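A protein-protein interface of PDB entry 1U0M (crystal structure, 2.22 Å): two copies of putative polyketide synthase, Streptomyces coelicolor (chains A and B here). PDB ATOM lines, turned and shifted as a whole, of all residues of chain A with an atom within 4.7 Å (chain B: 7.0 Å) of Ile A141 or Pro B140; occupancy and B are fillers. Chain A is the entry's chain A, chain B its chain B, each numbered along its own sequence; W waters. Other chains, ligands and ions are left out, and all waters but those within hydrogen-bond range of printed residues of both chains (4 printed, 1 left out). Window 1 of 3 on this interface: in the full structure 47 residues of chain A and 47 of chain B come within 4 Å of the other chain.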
ATOM      1  N   TYR A 111     -13.592  -4.075 -37.874  1.00  0.00           N
ATOM      2  CA  TYR A 111     -12.196  -4.200 -38.273  1.00  0.00           C
ATOM      3  C   TYR A 111     -11.525  -5.439 -37.692  1.00  0.00           C
ATOM      4  O   TYR A 111     -11.382  -5.555 -36.472  1.00  0.00           O
ATOM      5  CB  TYR A 111     -11.437  -2.948 -37.831  1.00  0.00           C
ATOM      6  CG  TYR A 111     -10.033  -2.818 -38.403  1.00  0.00           C
ATOM      7  CD1 TYR A 111      -9.805  -2.133 -39.599  1.00  0.00           C
ATOM      8  CD2 TYR A 111      -8.935  -3.372 -37.741  1.00  0.00           C
ATOM      9  CE1 TYR A 111      -8.519  -1.999 -40.114  1.00  0.00           C
ATOM     10  CE2 TYR A 111      -7.652  -3.242 -38.250  1.00  0.00           C
ATOM     11  CZ  TYR A 111      -7.449  -2.553 -39.433  1.00  0.00           C
ATOM     12  OH  TYR A 111      -6.171  -2.404 -39.916  1.00  0.00           O
ATOM     13  N   VAL A 112     -11.109  -6.365 -38.557  1.00  0.00           N
ATOM     14  CA  VAL A 112     -10.436  -7.572 -38.078  1.00  0.00           C
ATOM     15  C   VAL A 112      -8.989  -7.708 -38.550  1.00  0.00           C
ATOM     16  O   VAL A 112      -8.668  -7.545 -39.727  1.00  0.00           O
ATOM     17  CB  VAL A 112     -11.210  -8.843 -38.461  1.00  0.00           C
ATOM     18  CG1 VAL A 112     -12.595  -8.777 -37.861  1.00  0.00           C
ATOM     19  CG2 VAL A 112     -11.276  -8.989 -39.968  1.00  0.00           C
ATOM     20  N   SER A 113      -8.117  -7.999 -37.597  1.00  0.00           N
ATOM     21  CA  SER A 113      -6.697  -8.165 -37.860  1.00  0.00           C
ATOM     22  C   SER A 113      -6.028  -8.821 -36.669  1.00  0.00           C
ATOM     23  O   SER A 113      -6.285  -8.449 -35.527  1.00  0.00           O
ATOM     24  CB  SER A 113      -6.043  -6.814 -38.110  1.00  0.00           C
ATOM     25  OG  SER A 113      -4.634  -6.952 -38.094  1.00  0.00           O
ATOM     26  N   ILE A 139     -16.127  -1.993 -34.021  1.00  0.00           N
ATOM     27  CA  ILE A 139     -16.093  -3.348 -33.492  1.00  0.00           C
ATOM     28  C   ILE A 139     -14.799  -4.010 -33.942  1.00  0.00           C
ATOM     29  O   ILE A 139     -14.766  -4.732 -34.941  1.00  0.00           O
ATOM     30  CB  ILE A 139     -17.291  -4.193 -33.960  1.00  0.00           C
ATOM     31  CG1 ILE A 139     -18.589  -3.564 -33.455  1.00  0.00           C
ATOM     32  CG2 ILE A 139     -17.188  -5.603 -33.391  1.00  0.00           C
ATOM     33  CD1 ILE A 139     -19.817  -4.410 -33.701  1.00  0.00           C
ATOM     34  N   PRO A 140     -13.703  -3.737 -33.217  1.00  0.00           N
ATOM     35  CA  PRO A 140     -12.401  -4.313 -33.543  1.00  0.00           C
ATOM     36  C   PRO A 140     -12.202  -5.679 -32.896  1.00  0.00           C
ATOM     37  O   PRO A 140     -12.377  -5.836 -31.695  1.00  0.00           O
ATOM     38  CB  PRO A 140     -11.432  -3.267 -33.008  1.00  0.00           C
ATOM     39  CG  PRO A 140     -12.133  -2.786 -31.784  1.00  0.00           C
ATOM     40  CD  PRO A 140     -13.562  -2.644 -32.232  1.00  0.00           C
ATOM     41  N   ILE A 141     -11.857  -6.671 -33.700  1.00  0.00           N
ATOM     42  CA  ILE A 141     -11.607  -8.006 -33.176  1.00  0.00           C
ATOM     43  C   ILE A 141     -10.233  -8.481 -33.646  1.00  0.00           C
ATOM     44  O   ILE A 141     -10.016  -8.718 -34.836  1.00  0.00           O
ATOM     45  CB  ILE A 141     -12.668  -8.998 -33.646  1.00  0.00           C
ATOM     46  CG1 ILE A 141     -14.055  -8.473 -33.268  1.00  0.00           C
ATOM     47  CG2 ILE A 141     -12.415 -10.362 -33.006  1.00  0.00           C
ATOM     48  CD1 ILE A 141     -15.191  -9.398 -33.650  1.00  0.00           C
ATOM     49  N   ALA A 142      -9.301  -8.613 -32.710  1.00  0.00           N
ATOM     50  CA  ALA A 142      -7.955  -9.044 -33.062  1.00  0.00           C
ATOM     51  C   ALA A 142      -7.644 -10.479 -32.653  1.00  0.00           C
ATOM     52  O   ALA A 142      -6.616 -11.008 -33.032  1.00  0.00           O
ATOM     53  CB  ALA A 142      -6.930  -8.105 -32.435  1.00  0.00           C
ATOM     54  N   GLN A 143      -8.545 -11.118 -31.920  1.00  0.00           N
ATOM     55  CA  GLN A 143      -8.287 -12.462 -31.423  1.00  0.00           C
ATOM     56  C   GLN A 143      -8.990 -13.651 -32.067  1.00  0.00           C
ATOM     57  O   GLN A 143      -9.142 -14.684 -31.420  1.00  0.00           O
ATOM     58  CB  GLN A 143      -8.561 -12.475 -29.925  1.00  0.00           C
ATOM     59  CG  GLN A 143      -7.766 -11.442 -29.156  1.00  0.00           C
ATOM     60  CD  GLN A 143      -8.381 -11.112 -27.816  1.00  0.00           C
ATOM     61  OE1 GLN A 143      -9.385 -10.400 -27.738  1.00  0.00           O
ATOM     62  NE2 GLN A 143      -7.791 -11.629 -26.749  1.00  0.00           N
ATOM     63  N   LEU A 144      -9.399 -13.533 -33.328  1.00  0.00           N
ATOM     64  CA  LEU A 144     -10.073 -14.638 -34.005  1.00  0.00           C
ATOM     65  C   LEU A 144      -9.360 -15.157 -35.246  1.00  0.00           C
ATOM     66  O   LEU A 144      -9.891 -16.004 -35.960  1.00  0.00           O
ATOM     67  CB  LEU A 144     -11.511 -14.248 -34.345  1.00  0.00           C
ATOM     68  CG  LEU A 144     -12.435 -14.245 -33.119  1.00  0.00           C
ATOM     69  CD1 LEU A 144     -13.816 -13.758 -33.509  1.00  0.00           C
ATOM     70  CD2 LEU A 144     -12.505 -15.647 -32.533  1.00  0.00           C
ATOM     71  N   ILE B 109     -20.726 -14.837 -25.753  1.00  0.00           N
ATOM     72  CA  ILE B 109     -19.815 -14.331 -24.743  1.00  0.00           C
ATOM     73  C   ILE B 109     -19.066 -13.168 -25.356  1.00  0.00           C
ATOM     74  O   ILE B 109     -18.403 -13.310 -26.376  1.00  0.00           O
ATOM     75  CB  ILE B 109     -18.799 -15.383 -24.302  1.00  0.00           C
ATOM     76  CG1 ILE B 109     -19.522 -16.560 -23.654  1.00  0.00           C
ATOM     77  CG2 ILE B 109     -17.808 -14.763 -23.320  1.00  0.00           C
ATOM     78  CD1 ILE B 109     -18.618 -17.693 -23.255  1.00  0.00           C
ATOM     79  N   ILE B 110     -19.203 -12.007 -24.737  1.00  0.00           N
ATOM     80  CA  ILE B 110     -18.527 -10.802 -25.184  1.00  0.00           C
ATOM     81  C   ILE B 110     -17.425 -10.562 -24.166  1.00  0.00           C
ATOM     82  O   ILE B 110     -17.696 -10.120 -23.050  1.00  0.00           O
ATOM     83  CB  ILE B 110     -19.501  -9.628 -25.194  1.00  0.00           C
ATOM     84  CG1 ILE B 110     -20.715 -10.003 -26.051  1.00  0.00           C
ATOM     85  CG2 ILE B 110     -18.816  -8.389 -25.729  1.00  0.00           C
ATOM     86  CD1 ILE B 110     -21.817  -8.968 -26.057  1.00  0.00           C
ATOM     87  N   TYR B 111     -16.186 -10.864 -24.559  1.00  0.00           N
ATOM     88  CA  TYR B 111     -15.019 -10.740 -23.678  1.00  0.00           C
ATOM     89  C   TYR B 111     -14.145  -9.509 -23.934  1.00  0.00           C
ATOM     90  O   TYR B 111     -13.522  -9.393 -24.990  1.00  0.00           O
ATOM     91  CB  TYR B 111     -14.157 -11.997 -23.816  1.00  0.00           C
ATOM     92  CG  TYR B 111     -13.139 -12.193 -22.717  1.00  0.00           C
ATOM     93  CD1 TYR B 111     -13.472 -12.864 -21.542  1.00  0.00           C
ATOM     94  CD2 TYR B 111     -11.835 -11.708 -22.849  1.00  0.00           C
ATOM     95  CE1 TYR B 111     -12.532 -13.051 -20.529  1.00  0.00           C
ATOM     96  CE2 TYR B 111     -10.894 -11.886 -21.844  1.00  0.00           C
ATOM     97  CZ  TYR B 111     -11.246 -12.559 -20.689  1.00  0.00           C
ATOM     98  OH  TYR B 111     -10.308 -12.750 -19.701  1.00  0.00           O
ATOM     99  N   VAL B 112     -14.087  -8.603 -22.959  1.00  0.00           N
ATOM    100  CA  VAL B 112     -13.272  -7.391 -23.083  1.00  0.00           C
ATOM    101  C   VAL B 112     -12.098  -7.349 -22.092  1.00  0.00           C
ATOM    102  O   VAL B 112     -12.249  -7.639 -20.901  1.00  0.00           O
ATOM    103  CB  VAL B 112     -14.130  -6.115 -22.922  1.00  0.00           C
ATOM    104  CG1 VAL B 112     -15.163  -6.050 -24.043  1.00  0.00           C
ATOM    105  CG2 VAL B 112     -14.815  -6.101 -21.570  1.00  0.00           C
ATOM    106  N   SER B 113     -10.930  -6.989 -22.620  1.00  0.00           N
ATOM    107  CA  SER B 113      -9.690  -6.887 -21.863  1.00  0.00           C
ATOM    108  C   SER B 113      -8.610  -6.239 -22.737  1.00  0.00           C
ATOM    109  O   SER B 113      -8.442  -6.605 -23.899  1.00  0.00           O
ATOM    110  CB  SER B 113      -9.221  -8.275 -21.437  1.00  0.00           C
ATOM    111  OG  SER B 113      -7.894  -8.214 -20.953  1.00  0.00           O
ATOM    112  N   MET B 118      -4.056 -12.616 -25.976  1.00  0.00           N
ATOM    113  CA  MET B 118      -4.018 -14.029 -26.287  1.00  0.00           C
ATOM    114  C   MET B 118      -4.926 -14.367 -27.452  1.00  0.00           C
ATOM    115  O   MET B 118      -5.942 -13.714 -27.672  1.00  0.00           O
ATOM    116  CB  MET B 118      -4.346 -14.917 -25.057  1.00  0.00           C
ATOM    117  CG  MET B 118      -5.190 -14.323 -23.923  1.00  0.00           C
ATOM    118  SD  MET B 118      -5.191 -15.396 -22.383  1.00  0.00           S
ATOM    119  CE  MET B 118      -6.214 -16.816 -22.942  1.00  0.00           C
ATOM    120  N   MET B 119      -4.519 -15.359 -28.234  1.00  0.00           N
ATOM    121  CA  MET B 119      -5.321 -15.810 -29.353  1.00  0.00           C
ATOM    122  C   MET B 119      -5.201 -17.319 -29.435  1.00  0.00           C
ATOM    123  O   MET B 119      -4.111 -17.841 -29.627  1.00  0.00           O
ATOM    124  CB  MET B 119      -4.849 -15.211 -30.665  1.00  0.00           C
ATOM    125  CG  MET B 119      -5.587 -15.817 -31.840  1.00  0.00           C
ATOM    126  SD  MET B 119      -5.008 -15.226 -33.405  1.00  0.00           S
ATOM    127  CE  MET B 119      -6.085 -13.853 -33.602  1.00  0.00           C
ATOM    128  N   PRO B 120      -6.328 -18.035 -29.314  1.00  0.00           N
ATOM    129  CA  PRO B 120      -7.658 -17.461 -29.112  1.00  0.00           C
ATOM    130  C   PRO B 120      -7.760 -16.759 -27.760  1.00  0.00           C
ATOM    131  O   PRO B 120      -6.896 -16.951 -26.900  1.00  0.00           O
ATOM    132  CB  PRO B 120      -8.560 -18.686 -29.191  1.00  0.00           C
ATOM    133  CG  PRO B 120      -7.720 -19.729 -28.546  1.00  0.00           C
ATOM    134  CD  PRO B 120      -6.388 -19.507 -29.226  1.00  0.00           C
ATOM    135  N   SER B 121      -8.797 -15.936 -27.585  1.00  0.00           N
ATOM    136  CA  SER B 121      -9.002 -15.248 -26.313  1.00  0.00           C
ATOM    137  C   SER B 121      -9.519 -16.307 -25.350  1.00  0.00           C
ATOM    138  O   SER B 121      -9.737 -17.458 -25.751  1.00  0.00           O
ATOM    139  CB  SER B 121     -10.023 -14.123 -26.444  1.00  0.00           C
ATOM    140  OG  SER B 121     -11.306 -14.618 -26.773  1.00  0.00           O
ATOM    141  N   LEU B 122      -9.713 -15.922 -24.088  1.00  0.00           N
ATOM    142  CA  LEU B 122     -10.166 -16.846 -23.053  1.00  0.00           C
ATOM    143  C   LEU B 122     -11.576 -17.434 -23.259  1.00  0.00           C
ATOM    144  O   LEU B 122     -11.918 -18.428 -22.628  1.00  0.00           O
ATOM    145  CB  LEU B 122     -10.093 -16.169 -21.672  1.00  0.00           C
ATOM    146  CG  LEU B 122     -10.051 -17.121 -20.465  1.00  0.00           C
ATOM    147  CD1 LEU B 122      -8.631 -17.693 -20.299  1.00  0.00           C
ATOM    148  CD2 LEU B 122     -10.460 -16.371 -19.201  1.00  0.00           C
ATOM    149  N   THR B 123     -12.388 -16.830 -24.124  1.00  0.00           N
ATOM    150  CA  THR B 123     -13.740 -17.335 -24.362  1.00  0.00           C
ATOM    151  C   THR B 123     -13.732 -18.788 -24.821  1.00  0.00           C
ATOM    152  O   THR B 123     -14.599 -19.566 -24.435  1.00  0.00           O
ATOM    153  CB  THR B 123     -14.466 -16.529 -25.427  1.00  0.00           C
ATOM    154  OG1 THR B 123     -13.744 -16.628 -26.655  1.00  0.00           O
ATOM    155  CG2 THR B 123     -14.578 -15.073 -25.010  1.00  0.00           C
ATOM    156  N   GLN B 138     -18.678 -16.097 -29.722  1.00  0.00           N
ATOM    157  CA  GLN B 138     -17.647 -15.436 -28.934  1.00  0.00           C
ATOM    158  C   GLN B 138     -17.145 -14.136 -29.562  1.00  0.00           C
ATOM    159  O   GLN B 138     -16.552 -14.143 -30.637  1.00  0.00           O
ATOM    160  CB  GLN B 138     -16.478 -16.399 -28.677  1.00  0.00           C
ATOM    161  CG  GLN B 138     -16.141 -17.322 -29.832  1.00  0.00           C
ATOM    162  CD  GLN B 138     -15.047 -18.320 -29.492  1.00  0.00           C
ATOM    163  OE1 GLN B 138     -14.663 -19.137 -30.321  1.00  0.00           O
ATOM    164  NE2 GLN B 138     -14.543 -18.256 -28.271  1.00  0.00           N
ATOM    165  N   ILE B 139     -17.398 -13.021 -28.882  1.00  0.00           N
ATOM    166  CA  ILE B 139     -16.967 -11.713 -29.367  1.00  0.00           C
ATOM    167  C   ILE B 139     -15.907 -11.105 -28.441  1.00  0.00           C
ATOM    168  O   ILE B 139     -16.235 -10.476 -27.437  1.00  0.00           O
ATOM    169  CB  ILE B 139     -18.145 -10.730 -29.445  1.00  0.00           C
ATOM    170  CG1 ILE B 139     -19.255 -11.311 -30.313  1.00  0.00           C
ATOM    171  CG2 ILE B 139     -17.678  -9.401 -30.022  1.00  0.00           C
ATOM    172  CD1 ILE B 139     -20.429 -10.359 -30.504  1.00  0.00           C
ATOM    173  N   PRO B 140     -14.618 -11.306 -28.760  1.00  0.00           N
ATOM    174  CA  PRO B 140     -13.552 -10.754 -27.922  1.00  0.00           C
ATOM    175  C   PRO B 140     -13.042  -9.412 -28.444  1.00  0.00           C
ATOM    176  O   PRO B 140     -12.687  -9.293 -29.612  1.00  0.00           O
ATOM    177  CB  PRO B 140     -12.490 -11.837 -27.996  1.00  0.00           C
ATOM    178  CG  PRO B 140     -12.593 -12.258 -29.429  1.00  0.00           C
ATOM    179  CD  PRO B 140     -14.088 -12.353 -29.655  1.00  0.00           C
ATOM    180  N   ILE B 141     -13.013  -8.402 -27.585  1.00  0.00           N
ATOM    181  CA  ILE B 141     -12.529  -7.088 -27.994  1.00  0.00           C
ATOM    182  C   ILE B 141     -11.432  -6.592 -27.059  1.00  0.00           C
ATOM    183  O   ILE B 141     -11.658  -6.408 -25.864  1.00  0.00           O
ATOM    184  CB  ILE B 141     -13.663  -6.070 -28.010  1.00  0.00           C
ATOM    185  CG1 ILE B 141     -14.774  -6.568 -28.950  1.00  0.00           C
ATOM    186  CG2 ILE B 141     -13.122  -4.711 -28.454  1.00  0.00           C
ATOM    187  CD1 ILE B 141     -16.052  -5.751 -28.891  1.00  0.00           C
ATOM    188  N   ALA B 142     -10.245  -6.356 -27.612  1.00  0.00           N
ATOM    189  CA  ALA B 142      -9.108  -5.921 -26.809  1.00  0.00           C
ATOM    190  C   ALA B 142      -8.622  -4.508 -27.071  1.00  0.00           C
ATOM    191  O   ALA B 142      -7.779  -4.010 -26.336  1.00  0.00           O
ATOM    192  CB  ALA B 142      -7.940  -6.888 -27.025  1.00  0.00           C
ATOM    193  N   GLN B 143      -9.145  -3.869 -28.108  1.00  0.00           N
ATOM    194  CA  GLN B 143      -8.697  -2.535 -28.500  1.00  0.00           C
ATOM    195  C   GLN B 143      -9.597  -1.339 -28.168  1.00  0.00           C
ATOM    196  O   GLN B 143      -9.493  -0.291 -28.815  1.00  0.00           O
ATOM    197  CB  GLN B 143      -8.406  -2.557 -30.007  1.00  0.00           C
ATOM    198  CG  GLN B 143      -7.391  -3.626 -30.391  1.00  0.00           C
ATOM    199  CD  GLN B 143      -7.418  -4.000 -31.866  1.00  0.00           C
ATOM    200  OE1 GLN B 143      -8.319  -4.710 -32.341  1.00  0.00           O
ATOM    201  NE2 GLN B 143      -6.422  -3.532 -32.597  1.00  0.00           N
HETATM  202  O   HOH W   1     -11.278 -15.702 -29.376  1.00  0.00           O
HETATM  203  O   HOH W   2     -10.018  -9.227 -30.226  1.00  0.00           O
HETATM  204  O   HOH W   3      -9.910  -5.779 -30.347  1.00  0.00           O
HETATM  205  O   HOH W   4      -8.438  -5.269 -34.947  1.00  0.00           O
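The side-chain hydroxyl (OG1) of Thr B123 is in hydrogen-bond range of the side-chain hydroxyl (OG) of Ser B121 (3.2 Å). The backbone NH of Ser A113 lies within hydrogen-bond range of the backbone carbonyl oxygen of Ile A141 (3.4 Å). The side-chain amide nitrogen of Gln B138 is in hydrogen-bond range of the side-chain hydroxyl of Thr B123, 2.4 Å away. The backbone NH (N) of Ser B113 lies within hydrogen-bond range of the backbone carbonyl oxygen (O) of Ile B141 (3.4 Å). The backbone carbonyl oxygen (O) of Tyr A111 lies within hydrogen-bond range of the backbone NH (N) of Ile A141, 3.0 Å away. The backbone NH (N) of Ile B141 sits at hydrogen-bond distance from the backbone carbonyl oxygen (O) of Tyr B111, 2.8 Å away.
Among the printed residues, merely in contact across the chains: Ala A142 with Met B119, Gln A143 with Met B119, Leu A144 with Met B119, Gln A143 with Ser B121, Gln A143 with Pro B140, Pro A140 with Gln B143, Pro A140 with Ile B141, Ile A141 with Pro B140, Ala A142 with Gln B143, Gln A143 with Ala B142, Gln A143 with Pro B120 and Leu A144 with Gln B138.
Water W2 lies within hydrogen-bond range of N of Ala A142, O of Pro B140 and OE1 of Gln A143. Water W4 bridges OE1 of Gln B143 (2.7 Å) and O of Tyr A111 (3.3 Å). Water W3 lies within hydrogen-bond range of the side-chain amide oxygen (OE1) of Gln B143, the backbone carbonyl oxygen (O) of Pro A140 and the backbone NH (N) of Ala B142. Water W1 lies within hydrogen-bond range of OG of Ser B121 (2.8 Å) and O of Gln A143 (3.1 Å).
Hydrophobic or aromatic side chains of chain B within 4 Å of the printed part of chain A: Met B119, Pro B140, Ile B141 and Ala B142. Printed residues of chain A that touch a printed residue of chain B: Pro A140, Ile A141, Ala A142, Gln A143 and Leu A144. Hydrophobic or aromatic side chains of chain A within 4 Å of the printed part of chain B: Pro A140, Ile A141, Ala A142 and Leu A144. Among the printed residues, 13 pairs touch across the chains. Among the printed residues, no Asp or Glu carboxylate lies within 4 Å of a Lys or Arg side-chain nitrogen of the other chain.
Pro A140 touches Ile B141, and with the chains exchanged Ile A141 touches Pro B140. Pro A140 touches Gln B143, and with the chains exchanged Gln A143 touches Pro B140. Ala A142 touches Gln B143, and with the chains exchanged Gln A143 touches Ala B142. Positions printed for both chains: 111, 112, 113, 139, 140, 141, 142 and 143. Of the 13 pairs that touch across the chains among the printed residues, 6 have their exchanged pair printed and touching as well.
Of chain B, only Pro B140 comes within 4 Å of Ile A141. Printed residues of chain A within 4 Å of Pro B140: Ile A141 and Gln A143. Of the printed residues of chain A, Gln B143 touches Pro A140 and Ala A142. Of the printed residues of chain A, Ile B141 touches Pro A140. Of the printed residues of chain A, Ser B121 touches Gln A143. Printed residues of chain A within 4 Å of Ala B142: Gln A143. Of the printed residues of chain B, Leu A144 touches Met B119 and Gln B138. Ser B113 touches none of the printed residues of chain A. The nearest residue of chain B that does not touch Ile A141 is Gln B143 (4.3 Å). The nearest printed residue of chain A that does not touch Ile B141 is Gln A143 (4.1 Å).
The side-chain amide nitrogen (NE2) of Gln A143 is in hydrogen-bond range of the backbone carbonyl oxygen (O) of Met B118, 2.9 Å away.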
